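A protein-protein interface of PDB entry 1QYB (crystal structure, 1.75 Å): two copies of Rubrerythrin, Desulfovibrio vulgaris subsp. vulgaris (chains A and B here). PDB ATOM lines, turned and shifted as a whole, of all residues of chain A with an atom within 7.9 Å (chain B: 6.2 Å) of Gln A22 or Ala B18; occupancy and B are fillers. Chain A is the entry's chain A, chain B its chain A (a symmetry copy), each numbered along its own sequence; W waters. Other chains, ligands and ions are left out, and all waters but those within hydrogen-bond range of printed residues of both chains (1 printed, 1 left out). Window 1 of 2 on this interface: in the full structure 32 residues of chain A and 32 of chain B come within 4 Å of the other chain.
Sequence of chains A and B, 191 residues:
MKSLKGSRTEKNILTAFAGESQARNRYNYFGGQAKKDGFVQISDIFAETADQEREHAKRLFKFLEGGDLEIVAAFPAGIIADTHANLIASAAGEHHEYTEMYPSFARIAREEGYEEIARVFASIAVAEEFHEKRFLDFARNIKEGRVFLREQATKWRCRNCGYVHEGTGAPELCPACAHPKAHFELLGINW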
ATOM      1  N   THR A  15     -11.305 -13.356 -19.020  1.00  0.00           N
ATOM      2  CA  THR A  15     -10.877 -12.000 -18.697  1.00  0.00           C
ATOM      3  C   THR A  15      -9.922 -11.491 -19.771  1.00  0.00           C
ATOM      4  O   THR A  15     -10.008 -10.337 -20.189  1.00  0.00           O
ATOM      5  CB  THR A  15     -10.165 -11.940 -17.332  1.00  0.00           C
ATOM      6  OG1 THR A  15     -11.091 -12.290 -16.295  1.00  0.00           O
ATOM      7  CG2 THR A  15      -9.632 -10.540 -17.070  1.00  0.00           C
ATOM      8  N   ALA A  16      -9.013 -12.357 -20.209  1.00  0.00           N
ATOM      9  CA  ALA A  16      -8.051 -11.997 -21.249  1.00  0.00           C
ATOM     10  C   ALA A  16      -8.822 -11.725 -22.540  1.00  0.00           C
ATOM     11  O   ALA A  16      -8.536 -10.768 -23.262  1.00  0.00           O
ATOM     12  CB  ALA A  16      -7.049 -13.136 -21.456  1.00  0.00           C
ATOM     13  N   PHE A  17      -9.803 -12.574 -22.821  1.00  0.00           N
ATOM     14  CA  PHE A  17     -10.624 -12.419 -24.015  1.00  0.00           C
ATOM     15  C   PHE A  17     -11.359 -11.080 -23.983  1.00  0.00           C
ATOM     16  O   PHE A  17     -11.429 -10.379 -24.989  1.00  0.00           O
ATOM     17  CB  PHE A  17     -11.638 -13.563 -24.119  1.00  0.00           C
ATOM     18  CG  PHE A  17     -12.545 -13.460 -25.314  1.00  0.00           C
ATOM     19  CD1 PHE A  17     -12.061 -13.694 -26.597  1.00  0.00           C
ATOM     20  CD2 PHE A  17     -13.882 -13.110 -25.157  1.00  0.00           C
ATOM     21  CE1 PHE A  17     -12.901 -13.581 -27.715  1.00  0.00           C
ATOM     22  CE2 PHE A  17     -14.724 -12.995 -26.258  1.00  0.00           C
ATOM     23  CZ  PHE A  17     -14.233 -13.231 -27.544  1.00  0.00           C
ATOM     24  N   ALA A  18     -11.903 -10.723 -22.825  1.00  0.00           N
ATOM     25  CA  ALA A  18     -12.628  -9.460 -22.695  1.00  0.00           C
ATOM     26  C   ALA A  18     -11.690  -8.276 -22.922  1.00  0.00           C
ATOM     27  O   ALA A  18     -12.057  -7.292 -23.574  1.00  0.00           O
ATOM     28  CB  ALA A  18     -13.274  -9.364 -21.309  1.00  0.00           C
ATOM     29  N   GLY A  19     -10.476  -8.379 -22.384  1.00  0.00           N
ATOM     30  CA  GLY A  19      -9.504  -7.311 -22.538  1.00  0.00           C
ATOM     31  C   GLY A  19      -8.990  -7.191 -23.961  1.00  0.00           C
ATOM     32  O   GLY A  19      -8.853  -6.086 -24.491  1.00  0.00           O
ATOM     33  N   GLU A  20      -8.698  -8.329 -24.583  1.00  0.00           N
ATOM     34  CA  GLU A  20      -8.196  -8.330 -25.951  1.00  0.00           C
ATOM     35  C   GLU A  20      -9.267  -7.788 -26.888  1.00  0.00           C
ATOM     36  O   GLU A  20      -8.952  -7.106 -27.864  1.00  0.00           O
ATOM     37  CB  GLU A  20      -7.799  -9.749 -26.379  1.00  0.00           C
ATOM     38  CG  GLU A  20      -6.636 -10.347 -25.578  1.00  0.00           C
ATOM     39  CD  GLU A  20      -5.329  -9.591 -25.766  1.00  0.00           C
ATOM     40  OE1 GLU A  20      -5.320  -8.355 -25.592  1.00  0.00           O
ATOM     41  OE2 GLU A  20      -4.306 -10.235 -26.077  1.00  0.00           O
ATOM     42  N   SER A  21     -10.529  -8.086 -26.578  1.00  0.00           N
ATOM     43  CA  SER A  21     -11.659  -7.630 -27.387  1.00  0.00           C
ATOM     44  C   SER A  21     -11.785  -6.113 -27.347  1.00  0.00           C
ATOM     45  O   SER A  21     -12.046  -5.476 -28.367  1.00  0.00           O
ATOM     46  CB  SER A  21     -12.967  -8.260 -26.894  1.00  0.00           C
ATOM     47  OG  SER A  21     -12.992  -9.657 -27.119  1.00  0.00           O
ATOM     48  N   GLN A  22     -11.624  -5.534 -26.162  1.00  0.00           N
ATOM     49  CA  GLN A  22     -11.709  -4.087 -26.029  1.00  0.00           C
ATOM     50  C   GLN A  22     -10.496  -3.433 -26.683  1.00  0.00           C
ATOM     51  O   GLN A  22     -10.610  -2.366 -27.279  1.00  0.00           O
ATOM     52  CB  GLN A  22     -11.810  -3.696 -24.552  1.00  0.00           C
ATOM     53  CG  GLN A  22     -13.152  -4.063 -23.932  1.00  0.00           C
ATOM     54  CD  GLN A  22     -13.209  -3.774 -22.445  1.00  0.00           C
ATOM     55  OE1 GLN A  22     -13.013  -2.637 -22.011  1.00  0.00           O
ATOM     56  NE2 GLN A  22     -13.480  -4.808 -21.654  1.00  0.00           N
ATOM     57  N   ALA A  23      -9.337  -4.079 -26.587  1.00  0.00           N
ATOM     58  CA  ALA A  23      -8.126  -3.532 -27.194  1.00  0.00           C
ATOM     59  C   ALA A  23      -8.288  -3.470 -28.713  1.00  0.00           C
ATOM     60  O   ALA A  23      -7.822  -2.530 -29.355  1.00  0.00           O
ATOM     61  CB  ALA A  23      -6.897  -4.384 -26.822  1.00  0.00           C
ATOM     62  N   ARG A  24      -8.948  -4.469 -29.290  1.00  0.00           N
ATOM     63  CA  ARG A  24      -9.150  -4.472 -30.734  1.00  0.00           C
ATOM     64  C   ARG A  24      -9.932  -3.212 -31.128  1.00  0.00           C
ATOM     65  O   ARG A  24      -9.552  -2.502 -32.063  1.00  0.00           O
ATOM     66  CB  ARG A  24      -9.910  -5.727 -31.175  1.00  0.00           C
ATOM     67  CG  ARG A  24     -10.100  -5.814 -32.681  1.00  0.00           C
ATOM     68  CD  ARG A  24     -11.033  -6.946 -33.084  1.00  0.00           C
ATOM     69  NE  ARG A  24     -11.248  -6.917 -34.524  1.00  0.00           N
ATOM     70  CZ  ARG A  24     -12.162  -7.628 -35.170  1.00  0.00           C
ATOM     71  NH1 ARG A  24     -12.970  -8.447 -34.509  1.00  0.00           N
ATOM     72  NH2 ARG A  24     -12.275  -7.497 -36.486  1.00  0.00           N
ATOM     73  N   ASN A  25     -11.013  -2.921 -30.406  1.00  0.00           N
ATOM     74  CA  ASN A  25     -11.814  -1.735 -30.710  1.00  0.00           C
ATOM     75  C   ASN A  25     -11.000  -0.457 -30.491  1.00  0.00           C
ATOM     76  O   ASN A  25     -10.958   0.411 -31.363  1.00  0.00           O
ATOM     77  CB  ASN A  25     -13.085  -1.704 -29.845  1.00  0.00           C
ATOM     78  CG  ASN A  25     -14.255  -2.463 -30.473  1.00  0.00           C
ATOM     79  OD1 ASN A  25     -15.156  -2.938 -29.765  1.00  0.00           O
ATOM     80  ND2 ASN A  25     -14.264  -2.555 -31.799  1.00  0.00           N
ATOM     81  N   ARG A  26     -10.348  -0.342 -29.336  1.00  0.00           N
ATOM     82  CA  ARG A  26      -9.557   0.854 -29.055  1.00  0.00           C
ATOM     83  C   ARG A  26      -8.511   1.101 -30.143  1.00  0.00           C
ATOM     84  O   ARG A  26      -8.372   2.223 -30.627  1.00  0.00           O
ATOM     85  CB  ARG A  26      -8.858   0.751 -27.685  1.00  0.00           C
ATOM     86  CG  ARG A  26      -9.793   0.760 -26.470  1.00  0.00           C
ATOM     87  CD  ARG A  26      -9.026   1.105 -25.183  1.00  0.00           C
ATOM     88  NE  ARG A  26      -7.860   0.242 -24.978  1.00  0.00           N
ATOM     89  CZ  ARG A  26      -7.901  -0.966 -24.419  1.00  0.00           C
ATOM     90  NH1 ARG A  26      -9.051  -1.468 -23.995  1.00  0.00           N
ATOM     91  NH2 ARG A  26      -6.789  -1.680 -24.296  1.00  0.00           N
ATOM     92  N   TYR A  27      -7.781   0.061 -30.540  1.00  0.00           N
ATOM     93  CA  TYR A  27      -6.752   0.239 -31.564  1.00  0.00           C
ATOM     94  C   TYR A  27      -7.322   0.653 -32.916  1.00  0.00           C
ATOM     95  O   TYR A  27      -6.710   1.446 -33.637  1.00  0.00           O
ATOM     96  CB  TYR A  27      -5.895  -1.031 -31.701  1.00  0.00           C
ATOM     97  CG  TYR A  27      -5.088  -1.345 -30.454  1.00  0.00           C
ATOM     98  CD1 TYR A  27      -4.863  -0.371 -29.475  1.00  0.00           C
ATOM     99  CD2 TYR A  27      -4.527  -2.608 -30.266  1.00  0.00           C
ATOM    100  CE1 TYR A  27      -4.095  -0.652 -28.338  1.00  0.00           C
ATOM    101  CE2 TYR A  27      -3.762  -2.899 -29.138  1.00  0.00           C
ATOM    102  CZ  TYR A  27      -3.549  -1.919 -28.180  1.00  0.00           C
ATOM    103  OH  TYR A  27      -2.791  -2.221 -27.067  1.00  0.00           O
ATOM    104  N   ASN A  28      -8.489   0.129 -33.275  1.00  0.00           N
ATOM    105  CA  ASN A  28      -9.090   0.524 -34.542  1.00  0.00           C
ATOM    106  C   ASN A  28      -9.486   2.001 -34.461  1.00  0.00           C
ATOM    107  O   ASN A  28      -9.355   2.744 -35.434  1.00  0.00           O
ATOM    108  CB  ASN A  28     -10.317  -0.337 -34.859  1.00  0.00           C
ATOM    109  CG  ASN A  28      -9.965  -1.599 -35.635  1.00  0.00           C
ATOM    110  OD1 ASN A  28     -10.511  -2.667 -35.377  1.00  0.00           O
ATOM    111  ND2 ASN A  28      -9.056  -1.473 -36.603  1.00  0.00           N
ATOM    112  N   TYR A  29      -9.958   2.438 -33.296  1.00  0.00           N
ATOM    113  CA  TYR A  29     -10.350   3.833 -33.151  1.00  0.00           C
ATOM    114  C   TYR A  29      -9.121   4.723 -33.227  1.00  0.00           C
ATOM    115  O   TYR A  29      -9.154   5.768 -33.871  1.00  0.00           O
ATOM    116  CB  TYR A  29     -11.076   4.089 -31.825  1.00  0.00           C
ATOM    117  CG  TYR A  29     -12.252   3.179 -31.550  1.00  0.00           C
ATOM    118  CD1 TYR A  29     -12.981   2.599 -32.591  1.00  0.00           C
ATOM    119  CD2 TYR A  29     -12.631   2.889 -30.241  1.00  0.00           C
ATOM    120  CE1 TYR A  29     -14.056   1.742 -32.329  1.00  0.00           C
ATOM    121  CE2 TYR A  29     -13.702   2.043 -29.967  1.00  0.00           C
ATOM    122  CZ  TYR A  29     -14.407   1.471 -31.013  1.00  0.00           C
ATOM    123  OH  TYR A  29     -15.458   0.627 -30.730  1.00  0.00           O
ATOM    124  N   PHE A  30      -8.038   4.310 -32.572  1.00  0.00           N
ATOM    125  CA  PHE A  30      -6.808   5.098 -32.592  1.00  0.00           C
ATOM    126  C   PHE A  30      -6.256   5.115 -34.011  1.00  0.00           C
ATOM    127  O   PHE A  30      -5.595   6.069 -34.420  1.00  0.00           O
ATOM    128  CB  PHE A  30      -5.749   4.507 -31.649  1.00  0.00           C
ATOM    129  CG  PHE A  30      -6.151   4.495 -30.193  1.00  0.00           C
ATOM    130  CD1 PHE A  30      -7.105   5.384 -29.701  1.00  0.00           C
ATOM    131  CD2 PHE A  30      -5.538   3.614 -29.305  1.00  0.00           C
ATOM    132  CE1 PHE A  30      -7.444   5.393 -28.346  1.00  0.00           C
ATOM    133  CE2 PHE A  30      -5.864   3.613 -27.952  1.00  0.00           C
ATOM    134  CZ  PHE A  30      -6.820   4.504 -27.469  1.00  0.00           C
ATOM    135  N   GLU A  53      -4.881  -8.558 -32.226  1.00  0.00           N
ATOM    136  CA  GLU A  53      -5.560  -8.734 -30.942  1.00  0.00           C
ATOM    137  C   GLU A  53      -6.770  -9.644 -31.178  1.00  0.00           C
ATOM    138  O   GLU A  53      -7.140 -10.439 -30.308  1.00  0.00           O
ATOM    139  CB  GLU A  53      -6.038  -7.392 -30.379  1.00  0.00           C
ATOM    140  CG  GLU A  53      -4.935  -6.411 -30.058  1.00  0.00           C
ATOM    141  CD  GLU A  53      -4.047  -6.880 -28.926  1.00  0.00           C
ATOM    142  OE1 GLU A  53      -4.572  -7.133 -27.827  1.00  0.00           O
ATOM    143  OE2 GLU A  53      -2.829  -6.989 -29.136  1.00  0.00           O
ATOM    144  N   ALA A  57      -7.418 -13.110 -29.088  1.00  0.00           N
ATOM    145  CA  ALA A  57      -8.746 -13.363 -28.543  1.00  0.00           C
ATOM    146  C   ALA A  57      -9.349 -14.660 -29.084  1.00  0.00           C
ATOM    147  O   ALA A  57      -9.998 -15.404 -28.345  1.00  0.00           O
ATOM    148  CB  ALA A  57      -9.668 -12.189 -28.863  1.00  0.00           C
ATOM    149  N   ILE A  71     -17.135 -12.275 -14.598  1.00  0.00           N
ATOM    150  CA  ILE A  71     -15.751 -11.874 -14.396  1.00  0.00           C
ATOM    151  C   ILE A  71     -15.696 -10.525 -13.688  1.00  0.00           C
ATOM    152  O   ILE A  71     -16.643  -9.740 -13.747  1.00  0.00           O
ATOM    153  CB  ILE A  71     -14.982 -11.756 -15.736  1.00  0.00           C
ATOM    154  CG1 ILE A  71     -15.623 -10.676 -16.613  1.00  0.00           C
ATOM    155  CG2 ILE A  71     -14.971 -13.097 -16.445  1.00  0.00           C
ATOM    156  CD1 ILE A  71     -14.818 -10.335 -17.858  1.00  0.00           C
ATOM    157  N   ALA A  73     -13.006  -7.380 -13.456  1.00  0.00           N
ATOM    158  CA  ALA A  73     -11.759  -6.798 -13.926  1.00  0.00           C
ATOM    159  C   ALA A  73     -11.923  -5.324 -14.269  1.00  0.00           C
ATOM    160  O   ALA A  73     -13.037  -4.839 -14.472  1.00  0.00           O
ATOM    161  CB  ALA A  73     -11.253  -7.569 -15.147  1.00  0.00           C
ATOM    162  N   ALA A  74     -10.798  -4.620 -14.331  1.00  0.00           N
ATOM    163  CA  ALA A  74     -10.797  -3.200 -14.653  1.00  0.00           C
ATOM    164  C   ALA A  74     -10.307  -2.994 -16.079  1.00  0.00           C
ATOM    165  O   ALA A  74      -9.417  -3.701 -16.552  1.00  0.00           O
ATOM    166  CB  ALA A  74      -9.905  -2.441 -13.675  1.00  0.00           C
ATOM    167  N   PHE A  75     -10.893  -2.017 -16.760  1.00  0.00           N
ATOM    168  CA  PHE A  75     -10.525  -1.718 -18.137  1.00  0.00           C
ATOM    169  C   PHE A  75     -10.479  -0.207 -18.327  1.00  0.00           C
ATOM    170  O   PHE A  75     -11.040   0.547 -17.529  1.00  0.00           O
ATOM    171  CB  PHE A  75     -11.560  -2.310 -19.100  1.00  0.00           C
ATOM    172  CG  PHE A  75     -11.751  -3.795 -18.962  1.00  0.00           C
ATOM    173  CD1 PHE A  75     -10.793  -4.681 -19.444  1.00  0.00           C
ATOM    174  CD2 PHE A  75     -12.899  -4.307 -18.365  1.00  0.00           C
ATOM    175  CE1 PHE A  75     -10.977  -6.056 -19.339  1.00  0.00           C
ATOM    176  CE2 PHE A  75     -13.094  -5.679 -18.251  1.00  0.00           C
ATOM    177  CZ  PHE A  75     -12.130  -6.559 -18.741  1.00  0.00           C
ATOM    178  N   PRO A  76      -9.797   0.256 -19.385  1.00  0.00           N
ATOM    179  CA  PRO A  76      -9.706   1.693 -19.652  1.00  0.00           C
ATOM    180  C   PRO A  76     -11.062   2.264 -20.075  1.00  0.00           C
ATOM    181  O   PRO A  76     -11.616   1.870 -21.103  1.00  0.00           O
ATOM    182  CB  PRO A  76      -8.684   1.768 -20.786  1.00  0.00           C
ATOM    183  CG  PRO A  76      -7.839   0.552 -20.569  1.00  0.00           C
ATOM    184  CD  PRO A  76      -8.855  -0.497 -20.230  1.00  0.00           C
ATOM    185  N   ALA A  77     -11.609   3.174 -19.274  1.00  0.00           N
ATOM    186  CA  ALA A  77     -12.885   3.794 -19.612  1.00  0.00           C
ATOM    187  C   ALA A  77     -12.546   5.014 -20.465  1.00  0.00           C
ATOM    188  O   ALA A  77     -12.506   6.140 -19.970  1.00  0.00           O
ATOM    189  CB  ALA A  77     -13.625   4.218 -18.340  1.00  0.00           C
ATOM    190  N   GLY A  78     -12.308   4.780 -21.755  1.00  0.00           N
ATOM    191  CA  GLY A  78     -11.927   5.859 -22.651  1.00  0.00           C
ATOM    192  C   GLY A  78     -10.407   5.841 -22.708  1.00  0.00           C
ATOM    193  O   GLY A  78      -9.795   4.979 -22.074  1.00  0.00           O
ATOM    194  N   ILE B  13     -21.946   1.916 -19.093  1.00  0.00           N
ATOM    195  CA  ILE B  13     -21.395   2.209 -20.411  1.00  0.00           C
ATOM    196  C   ILE B  13     -20.180   1.318 -20.676  1.00  0.00           C
ATOM    197  O   ILE B  13     -20.047   0.737 -21.752  1.00  0.00           O
ATOM    198  CB  ILE B  13     -20.963   3.688 -20.532  1.00  0.00           C
ATOM    199  CG1 ILE B  13     -22.196   4.592 -20.485  1.00  0.00           C
ATOM    200  CG2 ILE B  13     -20.195   3.906 -21.839  1.00  0.00           C
ATOM    201  CD1 ILE B  13     -21.872   6.072 -20.506  1.00  0.00           C
ATOM    202  N   LEU B  14     -19.291   1.208 -19.696  1.00  0.00           N
ATOM    203  CA  LEU B  14     -18.114   0.371 -19.884  1.00  0.00           C
ATOM    204  C   LEU B  14     -18.528  -1.093 -20.035  1.00  0.00           C
ATOM    205  O   LEU B  14     -17.954  -1.824 -20.839  1.00  0.00           O
ATOM    206  CB  LEU B  14     -17.138   0.536 -18.713  1.00  0.00           C
ATOM    207  CG  LEU B  14     -15.834  -0.270 -18.798  1.00  0.00           C
ATOM    208  CD1 LEU B  14     -15.121   0.015 -20.115  1.00  0.00           C
ATOM    209  CD2 LEU B  14     -14.936   0.087 -17.620  1.00  0.00           C
ATOM    210  N   THR B  15     -19.535  -1.514 -19.273  1.00  0.00           N
ATOM    211  CA  THR B  15     -20.004  -2.893 -19.348  1.00  0.00           C
ATOM    212  C   THR B  15     -20.556  -3.175 -20.741  1.00  0.00           C
ATOM    213  O   THR B  15     -20.310  -4.237 -21.309  1.00  0.00           O
ATOM    214  CB  THR B  15     -21.109  -3.174 -18.311  1.00  0.00           C
ATOM    215  OG1 THR B  15     -20.567  -3.041 -16.990  1.00  0.00           O
ATOM    216  CG2 THR B  15     -21.656  -4.582 -18.484  1.00  0.00           C
ATOM    217  N   ALA B  16     -21.305  -2.218 -21.282  1.00  0.00           N
ATOM    218  CA  ALA B  16     -21.879  -2.359 -22.618  1.00  0.00           C
ATOM    219  C   ALA B  16     -20.733  -2.419 -23.627  1.00  0.00           C
ATOM    220  O   ALA B  16     -20.749  -3.224 -24.561  1.00  0.00           O
ATOM    221  CB  ALA B  16     -22.798  -1.173 -22.926  1.00  0.00           C
ATOM    222  N   PHE B  17     -19.738  -1.563 -23.429  1.00  0.00           N
ATOM    223  CA  PHE B  17     -18.579  -1.526 -24.310  1.00  0.00           C
ATOM    224  C   PHE B  17     -17.852  -2.871 -24.287  1.00  0.00           C
ATOM    225  O   PHE B  17     -17.448  -3.383 -25.328  1.00  0.00           O
ATOM    226  CB  PHE B  17     -17.618  -0.412 -23.884  1.00  0.00           C
ATOM    227  CG  PHE B  17     -16.377  -0.327 -24.730  1.00  0.00           C
ATOM    228  CD1 PHE B  17     -16.438   0.145 -26.037  1.00  0.00           C
ATOM    229  CD2 PHE B  17     -15.148  -0.739 -24.224  1.00  0.00           C
ATOM    230  CE1 PHE B  17     -15.286   0.209 -26.834  1.00  0.00           C
ATOM    231  CE2 PHE B  17     -13.999  -0.680 -25.006  1.00  0.00           C
ATOM    232  CZ  PHE B  17     -14.066  -0.205 -26.317  1.00  0.00           C
ATOM    233  N   ALA B  18     -17.691  -3.444 -23.100  1.00  0.00           N
ATOM    234  CA  ALA B  18     -17.008  -4.731 -22.975  1.00  0.00           C
ATOM    235  C   ALA B  18     -17.792  -5.828 -23.693  1.00  0.00           C
ATOM    236  O   ALA B  18     -17.209  -6.690 -24.360  1.00  0.00           O
ATOM    237  CB  ALA B  18     -16.830  -5.090 -21.496  1.00  0.00           C
ATOM    238  N   GLY B  19     -19.117  -5.787 -23.555  1.00  0.00           N
ATOM    239  CA  GLY B  19     -19.958  -6.782 -24.196  1.00  0.00           C
ATOM    240  C   GLY B  19     -19.994  -6.631 -25.706  1.00  0.00           C
ATOM    241  O   GLY B  19     -19.925  -7.620 -26.439  1.00  0.00           O
ATOM    242  N   GLU B  20     -20.107  -5.393 -26.176  1.00  0.00           N
ATOM    243  CA  GLU B  20     -20.152  -5.133 -27.609  1.00  0.00           C
ATOM    244  C   GLU B  20     -18.825  -5.531 -28.241  1.00  0.00           C
ATOM    245  O   GLU B  20     -18.796  -6.019 -29.371  1.00  0.00           O
ATOM    246  CB  GLU B  20     -20.435  -3.650 -27.881  1.00  0.00           C
ATOM    247  CG  GLU B  20     -21.808  -3.170 -27.394  1.00  0.00           C
ATOM    248  CD  GLU B  20     -22.966  -3.842 -28.116  1.00  0.00           C
ATOM    249  OE1 GLU B  20     -22.994  -5.090 -28.177  1.00  0.00           O
ATOM    250  OE2 GLU B  20     -23.858  -3.125 -28.614  1.00  0.00           O
ATOM    251  N   SER B  21     -17.735  -5.329 -27.501  1.00  0.00           N
ATOM    252  CA  SER B  21     -16.395  -5.667 -27.980  1.00  0.00           C
ATOM    253  C   SER B  21     -16.243  -7.170 -28.172  1.00  0.00           C
ATOM    254  O   SER B  21     -15.655  -7.623 -29.154  1.00  0.00           O
ATOM    255  CB  SER B  21     -15.327  -5.173 -26.995  1.00  0.00           C
ATOM    256  OG  SER B  21     -15.273  -3.759 -26.948  1.00  0.00           O
ATOM    257  N   GLN B  22     -16.753  -7.946 -27.221  1.00  0.00           N
ATOM    258  CA  GLN B  22     -16.672  -9.395 -27.329  1.00  0.00           C
ATOM    259  C   GLN B  22     -17.598  -9.887 -28.437  1.00  0.00           C
ATOM    260  O   GLN B  22     -17.270 -10.834 -29.146  1.00  0.00           O
ATOM    261  CB  GLN B  22     -17.031 -10.046 -25.989  1.00  0.00           C
ATOM    262  CG  GLN B  22     -15.965  -9.834 -24.923  1.00  0.00           C
ATOM    263  CD  GLN B  22     -16.371 -10.384 -23.570  1.00  0.00           C
ATOM    264  OE1 GLN B  22     -16.661 -11.574 -23.430  1.00  0.00           O
ATOM    265  NE2 GLN B  22     -16.393  -9.516 -22.563  1.00  0.00           N
ATOM    266  N   ALA B  23     -18.746  -9.235 -28.598  1.00  0.00           N
ATOM    267  CA  ALA B  23     -19.687  -9.630 -29.643  1.00  0.00           C
ATOM    268  C   ALA B  23     -19.052  -9.425 -31.019  1.00  0.00           C
ATOM    269  O   ALA B  23     -19.265 -10.221 -31.931  1.00  0.00           O
ATOM    270  CB  ALA B  23     -20.995  -8.822 -29.532  1.00  0.00           C
ATOM    271  N   ASN B  25     -15.918  -9.743 -31.835  1.00  0.00           N
ATOM    272  CA  ASN B  25     -15.028 -10.879 -32.077  1.00  0.00           C
ATOM    273  C   ASN B  25     -15.831 -12.151 -32.357  1.00  0.00           C
ATOM    274  O   ASN B  25     -15.571 -12.848 -33.337  1.00  0.00           O
ATOM    275  CB  ASN B  25     -14.094 -11.100 -30.875  1.00  0.00           C
ATOM    276  CG  ASN B  25     -12.809 -10.276 -30.956  1.00  0.00           C
ATOM    277  OD1 ASN B  25     -12.191  -9.961 -29.928  1.00  0.00           O
ATOM    278  ND2 ASN B  25     -12.384  -9.949 -32.173  1.00  0.00           N
ATOM    279  N   ILE B  71     -15.370  -3.533 -13.504  1.00  0.00           N
ATOM    280  CA  ILE B  71     -16.735  -3.924 -13.824  1.00  0.00           C
ATOM    281  C   ILE B  71     -16.971  -5.374 -13.421  1.00  0.00           C
ATOM    282  O   ILE B  71     -16.030  -6.164 -13.317  1.00  0.00           O
ATOM    283  CB  ILE B  71     -17.037  -3.779 -15.336  1.00  0.00           C
ATOM    284  CG1 ILE B  71     -16.122  -4.703 -16.144  1.00  0.00           C
ATOM    285  CG2 ILE B  71     -16.863  -2.333 -15.763  1.00  0.00           C
ATOM    286  CD1 ILE B  71     -16.483  -4.794 -17.619  1.00  0.00           C
ATOM    287  N   PHE B  75     -20.310 -13.057 -19.315  1.00  0.00           N
ATOM    288  CA  PHE B  75     -20.216 -13.095 -20.767  1.00  0.00           C
ATOM    289  C   PHE B  75     -20.156 -14.547 -21.227  1.00  0.00           C
ATOM    290  O   PHE B  75     -19.853 -15.446 -20.441  1.00  0.00           O
ATOM    291  CB  PHE B  75     -18.947 -12.372 -21.233  1.00  0.00           C
ATOM    292  CG  PHE B  75     -18.854 -10.942 -20.779  1.00  0.00           C
ATOM    293  CD1 PHE B  75     -19.635  -9.956 -21.374  1.00  0.00           C
ATOM    294  CD2 PHE B  75     -17.968 -10.577 -19.770  1.00  0.00           C
ATOM    295  CE1 PHE B  75     -19.534  -8.628 -20.972  1.00  0.00           C
ATOM    296  CE2 PHE B  75     -17.858  -9.253 -19.358  1.00  0.00           C
ATOM    297  CZ  PHE B  75     -18.643  -8.273 -19.962  1.00  0.00           C
HETATM  298  O   HOH W   1     -17.689  -3.895 -30.701  1.00  0.00           O
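The side-chain hydroxyl (OG) of Ser A21 lies within hydrogen-bond range of the side-chain amide oxygen (OD1) of Asn B25, 2.9 Å away.
NH1 of Arg A24 lies close to ND2 of Asn B25 (2.8 Å).
OD1 of Asn A25 lies within hydrogen-bond range of OG of Ser B21.
N of Ile B71 sits at hydrogen-bond distance from O of Ala A73 (2.8 Å).
O of Phe A17 lies within hydrogen-bond range of OG of Ser A21.
The backbone carbonyl oxygen of Ala A18 sits close to the side-chain amide nitrogen of Gln A22, 3.4 Å away.
The backbone carbonyl oxygen of Arg A24 sits close to the side-chain amide oxygen of Asn A28 (3.5 Å).
O of Phe B17 is in hydrogen-bond range of OG of Ser B21, at 2.7 Å.
NE2 of Gln B22 lies close to O of Ala B18 (3.4 Å).
Among the printed residues, merely in contact across the chains: Phe A17 with Gln B22 (3.6 Å), Phe A17 with Asn B25 (3.96 Å), Ala A18 with Gln B22 (3.4 Å), Ser A21 with Ser B21 (3.6 Å), Ser A21 with Gln B22 (3.7 Å), Gln A22 with Leu B14 (3.9 Å), Gln A22 with Phe B17 (3.6 Å), Gln A22 with Ala B18 (3.4 Å), Gln A22 with Ser B21 (3.7 Å), Asn A25 with Phe B17 (3.96 Å), Tyr A29 with Phe B17 (3.9 Å), Ala A57 with Asn B25 (3.5 Å), Ile A71 with Ile B71 (3.7 Å), Ile A71 with Phe B75 (3.6 Å), Phe A75 with Leu B14 (3.9 Å) and Phe A75 with Ile B71 (3.6 Å).
Printed residues of chain B within 4 Å of Gln A22: Leu B14, Phe B17, Ala B18 and Ser B21.
Of chain A, only Gln A22 (3.4 Å) comes within 4 Å of Ala B18.
No residue of chain A comes within 4 Å of Gly B19.
Of the printed residues of chain A, Ser B21 touches Ser A21 (3.6 Å), Gln A22 (3.7 Å) and Asn A25 (2.9 Å).
Printed residues of chain B within 4 Å of Ile A71: Ile B71 (3.7 Å) and Phe B75 (3.6 Å).
Of the printed residues of chain A, Gln B22 touches Phe A17, Ala A18 and Ser A21.
The nearest residue of chain B that does not touch Gln A22 is Ile B71 (5.0 Å).
The nearest residue of chain A that does not touch Ala B18 is Phe A75 (5.0 Å).
Of the 14 printed residues of chain B, 8 touch a printed residue of chain A.
Hydrophobic or aromatic side chains of chain B within 4 Å of the printed part of chain A: Leu B14, Phe B17, Ala B18, Ile B71 and Phe B75.
Printed residues of chain A that touch a printed residue of chain B: Phe A17, Ala A18, Ser A21, Gln A22, Arg A24, Asn A25, Tyr A29, Ala A57, Ile A71, Ala A73 and Phe A75.
Hydrophobic or aromatic side chains of chain A that line the printed part of chain B: Phe A17, Ala A18, Tyr A29, Ala A57, Ile A71 and Phe A75.
Among the printed residues, no Asp or Glu carboxylate lies within 4 Å of a Lys or Arg side-chain nitrogen of the other chain.
Ala A18 touches Gln B22, and with the chains exchanged Gln A22 touches Ala B18.
Ser A21 touches Gln B22, and with the chains exchanged Gln A22 touches Ser B21.
Ser A21 touches Asn B25, and with the chains exchanged Asn A25 touches Ser B21.
Ile B71 touches its own counterpart, Ile A71.
Of the 20 pairs that touch across the chains among the printed residues, 14 have their exchanged pair printed and touching as well.
Water W1 lies within hydrogen-bond range of the backbone carbonyl oxygen (O) of Glu B20 (2.7 Å) and the side-chain amide oxygen (OD1) of Asn A25 (2.9 Å).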
